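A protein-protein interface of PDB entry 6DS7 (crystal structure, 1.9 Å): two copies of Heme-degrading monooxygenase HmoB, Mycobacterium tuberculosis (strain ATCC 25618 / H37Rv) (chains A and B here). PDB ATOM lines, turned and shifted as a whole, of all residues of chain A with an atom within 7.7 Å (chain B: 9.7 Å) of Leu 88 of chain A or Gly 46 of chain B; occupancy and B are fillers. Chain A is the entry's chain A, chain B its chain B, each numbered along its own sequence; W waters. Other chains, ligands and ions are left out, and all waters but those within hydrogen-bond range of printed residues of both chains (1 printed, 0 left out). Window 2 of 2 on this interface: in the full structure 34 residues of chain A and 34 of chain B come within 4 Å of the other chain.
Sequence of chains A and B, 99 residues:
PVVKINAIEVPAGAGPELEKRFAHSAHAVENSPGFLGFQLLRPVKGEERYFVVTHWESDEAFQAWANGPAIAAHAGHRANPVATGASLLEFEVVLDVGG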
ATOM      1  N   VAL A   3      13.391  -2.903 -11.146  1.00  0.00           N
ATOM      2  CA  VAL A   3      12.203  -2.210 -11.627  1.00  0.00           C
ATOM      3  C   VAL A   3      12.339  -0.757 -11.231  1.00  0.00           C
ATOM      4  O   VAL A   3      12.721  -0.461 -10.090  1.00  0.00           O
ATOM      5  CB  VAL A   3      10.911  -2.828 -11.057  1.00  0.00           C
ATOM      6  CG1 VAL A   3       9.729  -1.886 -11.315  1.00  0.00           C
ATOM      7  CG2 VAL A   3      10.618  -4.179 -11.679  1.00  0.00           C
ATOM      8  N   LYS A   4      12.065   0.152 -12.173  1.00  0.00           N
ATOM      9  CA  LYS A   4      12.042   1.575 -11.885  1.00  0.00           C
ATOM     10  C   LYS A   4      10.665   2.090 -12.255  1.00  0.00           C
ATOM     11  O   LYS A   4      10.267   2.024 -13.429  1.00  0.00           O
ATOM     12  CB  LYS A   4      13.120   2.348 -12.669  1.00  0.00           C
ATOM     13  CG  LYS A   4      14.542   1.722 -12.657  1.00  0.00           C
ATOM     14  CD  LYS A   4      15.273   2.088 -11.395  1.00  0.00           C
ATOM     15  CE  LYS A   4      16.708   1.461 -11.374  1.00  0.00           C
ATOM     16  NZ  LYS A   4      17.201   1.322  -9.960  1.00  0.00           N
ATOM     17  N   ILE A   5       9.957   2.604 -11.265  1.00  0.00           N
ATOM     18  CA  ILE A   5       8.628   3.180 -11.457  1.00  0.00           C
ATOM     19  C   ILE A   5       8.694   4.699 -11.317  1.00  0.00           C
ATOM     20  O   ILE A   5       9.066   5.221 -10.253  1.00  0.00           O
ATOM     21  CB  ILE A   5       7.619   2.583 -10.464  1.00  0.00           C
ATOM     22  CG1 ILE A   5       7.668   1.033 -10.535  1.00  0.00           C
ATOM     23  CG2 ILE A   5       6.244   3.081 -10.800  1.00  0.00           C
ATOM     24  CD1 ILE A   5       6.679   0.357  -9.554  1.00  0.00           C
ATOM     25  N   ASN A   6       8.296   5.420 -12.371  1.00  0.00           N
ATOM     26  CA  ASN A   6       8.083   6.855 -12.226  1.00  0.00           C
ATOM     27  C   ASN A   6       6.615   7.052 -11.898  1.00  0.00           C
ATOM     28  O   ASN A   6       5.718   6.756 -12.719  1.00  0.00           O
ATOM     29  CB  ASN A   6       8.488   7.659 -13.460  1.00  0.00           C
ATOM     30  CG  ASN A   6       8.863   9.111 -13.105  1.00  0.00           C
ATOM     31  OD1 ASN A   6       9.491   9.332 -12.090  1.00  0.00           O
ATOM     32  ND2 ASN A   6       8.488  10.087 -13.953  1.00  0.00           N
ATOM     33  N   ALA A   7       6.379   7.539 -10.707  1.00  0.00           N
ATOM     34  CA  ALA A   7       5.035   7.765 -10.200  1.00  0.00           C
ATOM     35  C   ALA A   7       4.696   9.241 -10.449  1.00  0.00           C
ATOM     36  O   ALA A   7       5.291  10.153  -9.844  1.00  0.00           O
ATOM     37  CB  ALA A   7       4.950   7.385  -8.731  1.00  0.00           C
ATOM     38  N   ILE A   8       3.774   9.462 -11.376  1.00  0.00           N
ATOM     39  CA  ILE A   8       3.500  10.781 -11.961  1.00  0.00           C
ATOM     40  C   ILE A   8       2.191  11.337 -11.402  1.00  0.00           C
ATOM     41  O   ILE A   8       1.148  10.690 -11.530  1.00  0.00           O
ATOM     42  CB  ILE A   8       3.370  10.638 -13.483  1.00  0.00           C
ATOM     43  CG1 ILE A   8       4.666  10.251 -14.071  1.00  0.00           C
ATOM     44  CG2 ILE A   8       2.842  11.888 -14.084  1.00  0.00           C
ATOM     45  CD1 ILE A   8       5.695  10.981 -13.393  1.00  0.00           C
ATOM     46  N   ARG A  49      -1.788   8.528  -8.707  1.00  0.00           N
ATOM     47  CA  ARG A  49      -0.703   8.755  -9.657  1.00  0.00           C
ATOM     48  C   ARG A  49      -0.703   7.720 -10.778  1.00  0.00           C
ATOM     49  O   ARG A  49      -1.021   6.564 -10.565  1.00  0.00           O
ATOM     50  CB  ARG A  49       0.661   8.700  -8.931  1.00  0.00           C
ATOM     51  CG  ARG A  49       0.781   9.789  -7.915  1.00  0.00           C
ATOM     52  CD  ARG A  49       2.056   9.642  -7.102  1.00  0.00           C
ATOM     53  NE  ARG A  49       2.013   8.399  -6.333  1.00  0.00           N
ATOM     54  CZ  ARG A  49       3.014   7.972  -5.567  1.00  0.00           C
ATOM     55  NH1 ARG A  49       4.120   8.688  -5.469  1.00  0.00           N
ATOM     56  NH2 ARG A  49       2.895   6.837  -4.893  1.00  0.00           N
ATOM     57  N   VAL A  52       4.586   4.669 -14.343  1.00  0.00           N
ATOM     58  CA  VAL A  52       5.364   4.266 -15.510  1.00  0.00           C
ATOM     59  C   VAL A  52       6.354   3.211 -15.018  1.00  0.00           C
ATOM     60  O   VAL A  52       7.348   3.517 -14.341  1.00  0.00           O
ATOM     61  CB  VAL A  52       6.075   5.462 -16.158  1.00  0.00           C
ATOM     62  CG1 VAL A  52       6.787   5.006 -17.451  1.00  0.00           C
ATOM     63  CG2 VAL A  52       5.055   6.581 -16.451  1.00  0.00           C
ATOM     64  N   THR A  54       9.039   0.419 -15.489  1.00  0.00           N
ATOM     65  CA  THR A  54      10.047  -0.083 -16.405  1.00  0.00           C
ATOM     66  C   THR A  54      10.864  -1.187 -15.727  1.00  0.00           C
ATOM     67  O   THR A  54      11.155  -1.143 -14.526  1.00  0.00           O
ATOM     68  CB  THR A  54      10.983   1.040 -16.890  1.00  0.00           C
ATOM     69  OG1 THR A  54      11.810   1.498 -15.804  1.00  0.00           O
ATOM     70  CG2 THR A  54      10.118   2.228 -17.403  1.00  0.00           C
ATOM     71  N   ASP A  59      20.611  -2.029 -12.922  1.00  0.00           N
ATOM     72  CA  ASP A  59      20.593  -0.590 -12.685  1.00  0.00           C
ATOM     73  C   ASP A  59      21.437   0.172 -13.720  1.00  0.00           C
ATOM     74  O   ASP A  59      21.004   1.221 -14.240  1.00  0.00           O
ATOM     75  CB  ASP A  59      21.069  -0.320 -11.253  1.00  0.00           C
ATOM     76  CG  ASP A  59      20.898   1.132 -10.847  1.00  0.00           C
ATOM     77  OD1 ASP A  59      19.735   1.593 -10.802  1.00  0.00           O
ATOM     78  OD2 ASP A  59      21.919   1.806 -10.558  1.00  0.00           O
ATOM     79  N   PHE A  62      19.502   0.895 -16.985  1.00  0.00           N
ATOM     80  CA  PHE A  62      18.573   2.014 -16.860  1.00  0.00           C
ATOM     81  C   PHE A  62      19.300   3.355 -16.892  1.00  0.00           C
ATOM     82  O   PHE A  62      18.865   4.287 -17.588  1.00  0.00           O
ATOM     83  CB  PHE A  62      17.765   1.887 -15.567  1.00  0.00           C
ATOM     84  CG  PHE A  62      17.138   3.155 -15.150  1.00  0.00           C
ATOM     85  CD1 PHE A  62      16.057   3.663 -15.858  1.00  0.00           C
ATOM     86  CD2 PHE A  62      17.667   3.901 -14.085  1.00  0.00           C
ATOM     87  CE1 PHE A  62      15.480   4.888 -15.488  1.00  0.00           C
ATOM     88  CE2 PHE A  62      17.082   5.130 -13.705  1.00  0.00           C
ATOM     89  CZ  PHE A  62      15.987   5.615 -14.409  1.00  0.00           C
ATOM     90  N   GLN A  63      20.374   3.486 -16.093  1.00  0.00           N
ATOM     91  CA  GLN A  63      21.156   4.729 -16.044  1.00  0.00           C
ATOM     92  C   GLN A  63      21.714   5.094 -17.413  1.00  0.00           C
ATOM     93  O   GLN A  63      21.664   6.265 -17.812  1.00  0.00           O
ATOM     94  CB  GLN A  63      22.302   4.605 -15.038  1.00  0.00           C
ATOM     95  CG  GLN A  63      21.844   4.012 -13.715  1.00  0.00           C
ATOM     96  CD  GLN A  63      22.033   4.920 -12.544  1.00  0.00           C
ATOM     97  OE1 GLN A  63      21.373   5.949 -12.431  1.00  0.00           O
ATOM     98  NE2 GLN A  63      22.919   4.525 -11.632  1.00  0.00           N
ATOM     99  N   ALA A  86       6.601  14.203  -9.787  1.00  0.00           N
ATOM    100  CA  ALA A  86       6.999  12.864 -10.168  1.00  0.00           C
ATOM    101  C   ALA A  86       7.918  12.329  -9.096  1.00  0.00           C
ATOM    102  O   ALA A  86       8.713  13.076  -8.540  1.00  0.00           O
ATOM    103  CB  ALA A  86       7.726  12.828 -11.517  1.00  0.00           C
ATOM    104  N   SER A  87       7.808  11.026  -8.810  1.00  0.00           N
ATOM    105  CA  SER A  87       8.689  10.377  -7.839  1.00  0.00           C
ATOM    106  C   SER A  87       9.142   9.060  -8.445  1.00  0.00           C
ATOM    107  O   SER A  87       8.305   8.275  -8.906  1.00  0.00           O
ATOM    108  CB  SER A  87       8.001  10.077  -6.482  1.00  0.00           C
ATOM    109  OG  SER A  87       7.251  11.153  -6.009  1.00  0.00           O
ATOM    110  N   LEU A  88      10.440   8.830  -8.434  1.00  0.00           N
ATOM    111  CA  LEU A  88      11.033   7.605  -8.942  1.00  0.00           C
ATOM    112  C   LEU A  88      11.102   6.573  -7.818  1.00  0.00           C
ATOM    113  O   LEU A  88      11.738   6.811  -6.789  1.00  0.00           O
ATOM    114  CB  LEU A  88      12.428   7.873  -9.488  1.00  0.00           C
ATOM    115  CG  LEU A  88      13.053   6.635 -10.120  1.00  0.00           C
ATOM    116  CD1 LEU A  88      12.312   6.211 -11.362  1.00  0.00           C
ATOM    117  CD2 LEU A  88      14.533   6.861 -10.436  1.00  0.00           C
ATOM    118  N   LEU A  89      10.468   5.428  -8.021  1.00  0.00           N
ATOM    119  CA  LEU A  89      10.490   4.326  -7.073  1.00  0.00           C
ATOM    120  C   LEU A  89      11.339   3.207  -7.651  1.00  0.00           C
ATOM    121  O   LEU A  89      11.105   2.757  -8.776  1.00  0.00           O
ATOM    122  CB  LEU A  89       9.064   3.786  -6.774  1.00  0.00           C
ATOM    123  CG  LEU A  89       7.960   4.816  -6.683  1.00  0.00           C
ATOM    124  CD1 LEU A  89       6.580   4.183  -6.385  1.00  0.00           C
ATOM    125  CD2 LEU A  89       8.268   5.868  -5.606  1.00  0.00           C
ATOM    126  N   GLU A  90      12.365   2.821  -6.900  1.00  0.00           N
ATOM    127  CA  GLU A  90      13.339   1.822  -7.396  1.00  0.00           C
ATOM    128  C   GLU A  90      13.242   0.533  -6.588  1.00  0.00           C
ATOM    129  O   GLU A  90      13.212   0.603  -5.361  1.00  0.00           O
ATOM    130  CB  GLU A  90      14.739   2.419  -7.346  1.00  0.00           C
ATOM    131  CG  GLU A  90      14.794   3.771  -8.013  1.00  0.00           C
ATOM    132  CD  GLU A  90      16.195   4.309  -8.209  1.00  0.00           C
ATOM    133  OE1 GLU A  90      16.492   5.366  -7.643  1.00  0.00           O
ATOM    134  OE2 GLU A  90      16.975   3.659  -8.925  1.00  0.00           O
ATOM    135  N   PHE A  91      13.240  -0.593  -7.293  1.00  0.00           N
ATOM    136  CA  PHE A  91      13.127  -1.905  -6.625  1.00  0.00           C
ATOM    137  C   PHE A  91      14.017  -2.931  -7.320  1.00  0.00           C
ATOM    138  O   PHE A  91      14.468  -2.711  -8.451  1.00  0.00           O
ATOM    139  CB  PHE A  91      11.708  -2.449  -6.789  1.00  0.00           C
ATOM    140  CG  PHE A  91      10.597  -1.588  -6.254  1.00  0.00           C
ATOM    141  CD1 PHE A  91      10.049  -0.579  -7.022  1.00  0.00           C
ATOM    142  CD2 PHE A  91      10.068  -1.818  -4.997  1.00  0.00           C
ATOM    143  CE1 PHE A  91       9.006   0.192  -6.538  1.00  0.00           C
ATOM    144  CE2 PHE A  91       9.035  -1.036  -4.507  1.00  0.00           C
ATOM    145  CZ  PHE A  91       8.502  -0.036  -5.282  1.00  0.00           C
ATOM    146  N   ARG B  42      11.381  -5.862  -4.075  1.00  0.00           N
ATOM    147  CA  ARG B  42      11.994  -5.381  -2.841  1.00  0.00           C
ATOM    148  C   ARG B  42      12.414  -3.928  -3.018  1.00  0.00           C
ATOM    149  O   ARG B  42      13.161  -3.629  -3.948  1.00  0.00           O
ATOM    150  CB  ARG B  42      13.229  -6.203  -2.500  1.00  0.00           C
ATOM    151  CG  ARG B  42      14.016  -5.619  -1.310  1.00  0.00           C
ATOM    152  CD  ARG B  42      15.483  -6.126  -1.292  1.00  0.00           C
ATOM    153  NE  ARG B  42      15.526  -7.588  -1.193  1.00  0.00           N
ATOM    154  CZ  ARG B  42      16.504  -8.340  -1.703  1.00  0.00           C
ATOM    155  NH1 ARG B  42      17.516  -7.755  -2.367  1.00  0.00           N
ATOM    156  NH2 ARG B  42      16.476  -9.660  -1.552  1.00  0.00           N
ATOM    157  N   PRO B  43      11.990  -3.017  -2.137  1.00  0.00           N
ATOM    158  CA  PRO B  43      12.277  -1.590  -2.345  1.00  0.00           C
ATOM    159  C   PRO B  43      13.748  -1.268  -2.118  1.00  0.00           C
ATOM    160  O   PRO B  43      14.361  -1.787  -1.188  1.00  0.00           O
ATOM    161  CB  PRO B  43      11.428  -0.910  -1.282  1.00  0.00           C
ATOM    162  CG  PRO B  43      11.386  -1.892  -0.180  1.00  0.00           C
ATOM    163  CD  PRO B  43      11.363  -3.270  -0.838  1.00  0.00           C
ATOM    164  N   VAL B  44      14.277  -0.339  -2.931  1.00  0.00           N
ATOM    165  CA  VAL B  44      15.686   0.031  -2.909  1.00  0.00           C
ATOM    166  C   VAL B  44      15.855   1.516  -2.646  1.00  0.00           C
ATOM    167  O   VAL B  44      16.738   1.917  -1.888  1.00  0.00           O
ATOM    168  CB  VAL B  44      16.386  -0.377  -4.236  1.00  0.00           C
ATOM    169  CG1 VAL B  44      17.720   0.362  -4.452  1.00  0.00           C
ATOM    170  CG2 VAL B  44      16.562  -1.929  -4.304  1.00  0.00           C
ATOM    171  N   LYS B  45      15.008   2.341  -3.262  1.00  0.00           N
ATOM    172  CA  LYS B  45      15.034   3.783  -3.087  1.00  0.00           C
ATOM    173  C   LYS B  45      13.648   4.332  -3.396  1.00  0.00           C
ATOM    174  O   LYS B  45      12.986   3.845  -4.304  1.00  0.00           O
ATOM    175  CB  LYS B  45      16.074   4.427  -4.008  1.00  0.00           C
ATOM    176  CG  LYS B  45      16.314   5.909  -3.748  1.00  0.00           C
ATOM    177  CD  LYS B  45      17.373   6.461  -4.722  1.00  0.00           C
ATOM    178  CE  LYS B  45      18.097   7.700  -4.182  1.00  0.00           C
ATOM    179  NZ  LYS B  45      19.105   7.381  -3.098  1.00  0.00           N
ATOM    180  N   GLY B  46      13.220   5.328  -2.623  1.00  0.00           N
ATOM    181  CA  GLY B  46      12.009   6.054  -2.896  1.00  0.00           C
ATOM    182  C   GLY B  46      10.746   5.436  -2.341  1.00  0.00           C
ATOM    183  O   GLY B  46       9.691   6.082  -2.369  1.00  0.00           O
ATOM    184  N   GLU B  47      10.830   4.235  -1.792  1.00  0.00           N
ATOM    185  CA  GLU B  47       9.669   3.522  -1.282  1.00  0.00           C
ATOM    186  C   GLU B  47      10.181   2.629  -0.164  1.00  0.00           C
ATOM    187  O   GLU B  47      11.324   2.165  -0.214  1.00  0.00           O
ATOM    188  CB  GLU B  47       8.995   2.759  -2.454  1.00  0.00           C
ATOM    189  CG  GLU B  47       7.800   1.881  -2.158  1.00  0.00           C
ATOM    190  CD  GLU B  47       6.645   2.604  -1.475  1.00  0.00           C
ATOM    191  OE1 GLU B  47       5.930   3.405  -2.133  1.00  0.00           O
ATOM    192  OE2 GLU B  47       6.457   2.352  -0.270  1.00  0.00           O
ATOM    193  N   GLU B  48       9.361   2.388   0.857  1.00  0.00           N
ATOM    194  CA  GLU B  48       9.821   1.504   1.961  1.00  0.00           C
ATOM    195  C   GLU B  48       9.009   0.210   1.948  1.00  0.00           C
ATOM    196  O   GLU B  48       9.386  -0.729   2.655  1.00  0.00           O
ATOM    197  CB  GLU B  48       9.650   2.197   3.311  1.00  0.00           C
ATOM    198  CG  GLU B  48       9.543   3.702   3.201  1.00  0.00           C
ATOM    199  CD  GLU B  48      10.224   4.443   4.335  1.00  0.00           C
ATOM    200  OE1 GLU B  48      11.244   5.108   4.075  1.00  0.00           O
ATOM    201  OE2 GLU B  48       9.728   4.351   5.472  1.00  0.00           O
ATOM    202  N   ARG B  49       7.949   0.172   1.144  1.00  0.00           N
ATOM    203  CA  ARG B  49       7.067  -1.018   1.105  1.00  0.00           C
ATOM    204  C   ARG B  49       7.494  -1.982   0.000  1.00  0.00           C
ATOM    205  O   ARG B  49       8.124  -1.543  -0.970  1.00  0.00           O
ATOM    206  CB  ARG B  49       5.629  -0.580   0.829  1.00  0.00           C
ATOM    207  CG  ARG B  49       5.025   0.277   1.927  1.00  0.00           C
ATOM    208  CD  ARG B  49       3.678   0.819   1.514  1.00  0.00           C
ATOM    209  NE  ARG B  49       3.727   1.653   0.327  1.00  0.00           N
ATOM    210  CZ  ARG B  49       2.667   2.250  -0.195  1.00  0.00           C
ATOM    211  NH1 ARG B  49       1.501   2.146   0.411  1.00  0.00           N
ATOM    212  NH2 ARG B  49       2.774   2.934  -1.321  1.00  0.00           N
ATOM    213  N   PHE B  51       6.477  -4.188  -3.143  1.00  0.00           N
ATOM    214  CA  PHE B  51       5.399  -4.162  -4.123  1.00  0.00           C
ATOM    215  C   PHE B  51       5.168  -5.582  -4.625  1.00  0.00           C
ATOM    216  O   PHE B  51       6.088  -6.223  -5.136  1.00  0.00           O
ATOM    217  CB  PHE B  51       5.719  -3.248  -5.316  1.00  0.00           C
ATOM    218  CG  PHE B  51       5.352  -1.815  -5.110  1.00  0.00           C
ATOM    219  CD1 PHE B  51       5.118  -1.304  -3.831  1.00  0.00           C
ATOM    220  CD2 PHE B  51       5.244  -0.952  -6.210  1.00  0.00           C
ATOM    221  CE1 PHE B  51       4.841   0.043  -3.634  1.00  0.00           C
ATOM    222  CE2 PHE B  51       4.925   0.392  -6.003  1.00  0.00           C
ATOM    223  CZ  PHE B  51       4.719   0.881  -4.722  1.00  0.00           C
HETATM  224  O   HOH W   1       4.917   5.992  -2.976  1.00  0.00           O
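The backbone NH (N) of Val 44 of chain B sits at hydrogen-bond distance from the backbone carbonyl oxygen (O) of Glu 90 of chain A (2.8 Å).
The backbone NH (N) of Glu 90 of chain A is in hydrogen-bond range of the backbone carbonyl oxygen (O) of Lys 45 of chain B (2.9 Å).
The backbone NH of Phe 91 of chain A lies within hydrogen-bond range of the backbone carbonyl oxygen of Val 3 of chain A (2.8 Å).
OE2 of Glu 90 of chain A lies within salt-bridge range of NZ of Lys 4 of chain A.
The backbone carbonyl oxygen (O) of Ile 5 of chain A is in hydrogen-bond range of the backbone NH (N) of Leu 89 of chain A (2.6 Å).
The side-chain carboxylate (OE2) of Glu 47 of chain B lies within salt-bridge range of the guanidinium group (NE) of Arg 49 of chain B (2.9 Å).
CD1 of Ile 5 of chain A touches CD2 of Phe 51 of chain B (3.9 Å).
O of Leu 88 of chain A touches CA of Gly 46 of chain B, at 3.98 Å.
O of Lys 45 of chain B touches CA of Leu 89 of chain A, 3.8 Å away.
Gly 46 of chain B touches Leu 89 of chain A (O to CD2, 3.5 Å).
O of Glu 90 of chain A touches C of Pro 43 of chain B, at 3.8 Å.
Arg 42 of chain B touches Phe 91 of chain A.
CA of Pro 43 of chain B touches CD2 of Phe 91 of chain A (3.5 Å).
CZ of Phe 91 of chain A touches CG of Glu 47 of chain B (3.7 Å).
Arg 49 of chain B touches Phe 91 of chain A (O to CE2, 3.7 Å).
CZ of Phe 91 of chain A touches CD2 of Phe 51 of chain B (3.5 Å).
Of chain B, only Gly 46 (3.98 Å) comes within 4 Å of Leu 88 of chain A.
Gly 46 of chain B touches two residues of chain A.
No residue of chain B comes within 4 Å of Ser 87 of chain A.
Of the printed residues of chain B, Leu 89 of chain A touches Lys 45 and Gly 46.
Printed residues of chain A within 4 Å of Lys 45 of chain B: Leu 89 and Glu 90.
Of the printed residues of chain B, Glu 90 of chain A touches Pro 43, Val 44 and Lys 45.
Of the printed residues of chain A, Arg 42 of chain B touches Phe 91.
The nearest printed residue of chain A that does not touch Phe 51 of chain B is Leu 89 of chain A (4.1 Å).
Hydrophobic or aromatic side chains of chain A within 4 Å of the printed part of chain B: Ile 5, Leu 89 and Phe 91.
Hydrophobic or aromatic side chains of chain B that line the printed part of chain A: Val 44 and Phe 51.
Position printed for both chains: 49.
Water W1 lies within hydrogen-bond range of the side-chain carboxylate of Glu 47 of chain B and the guanidinium group of Arg 49 of chain A.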
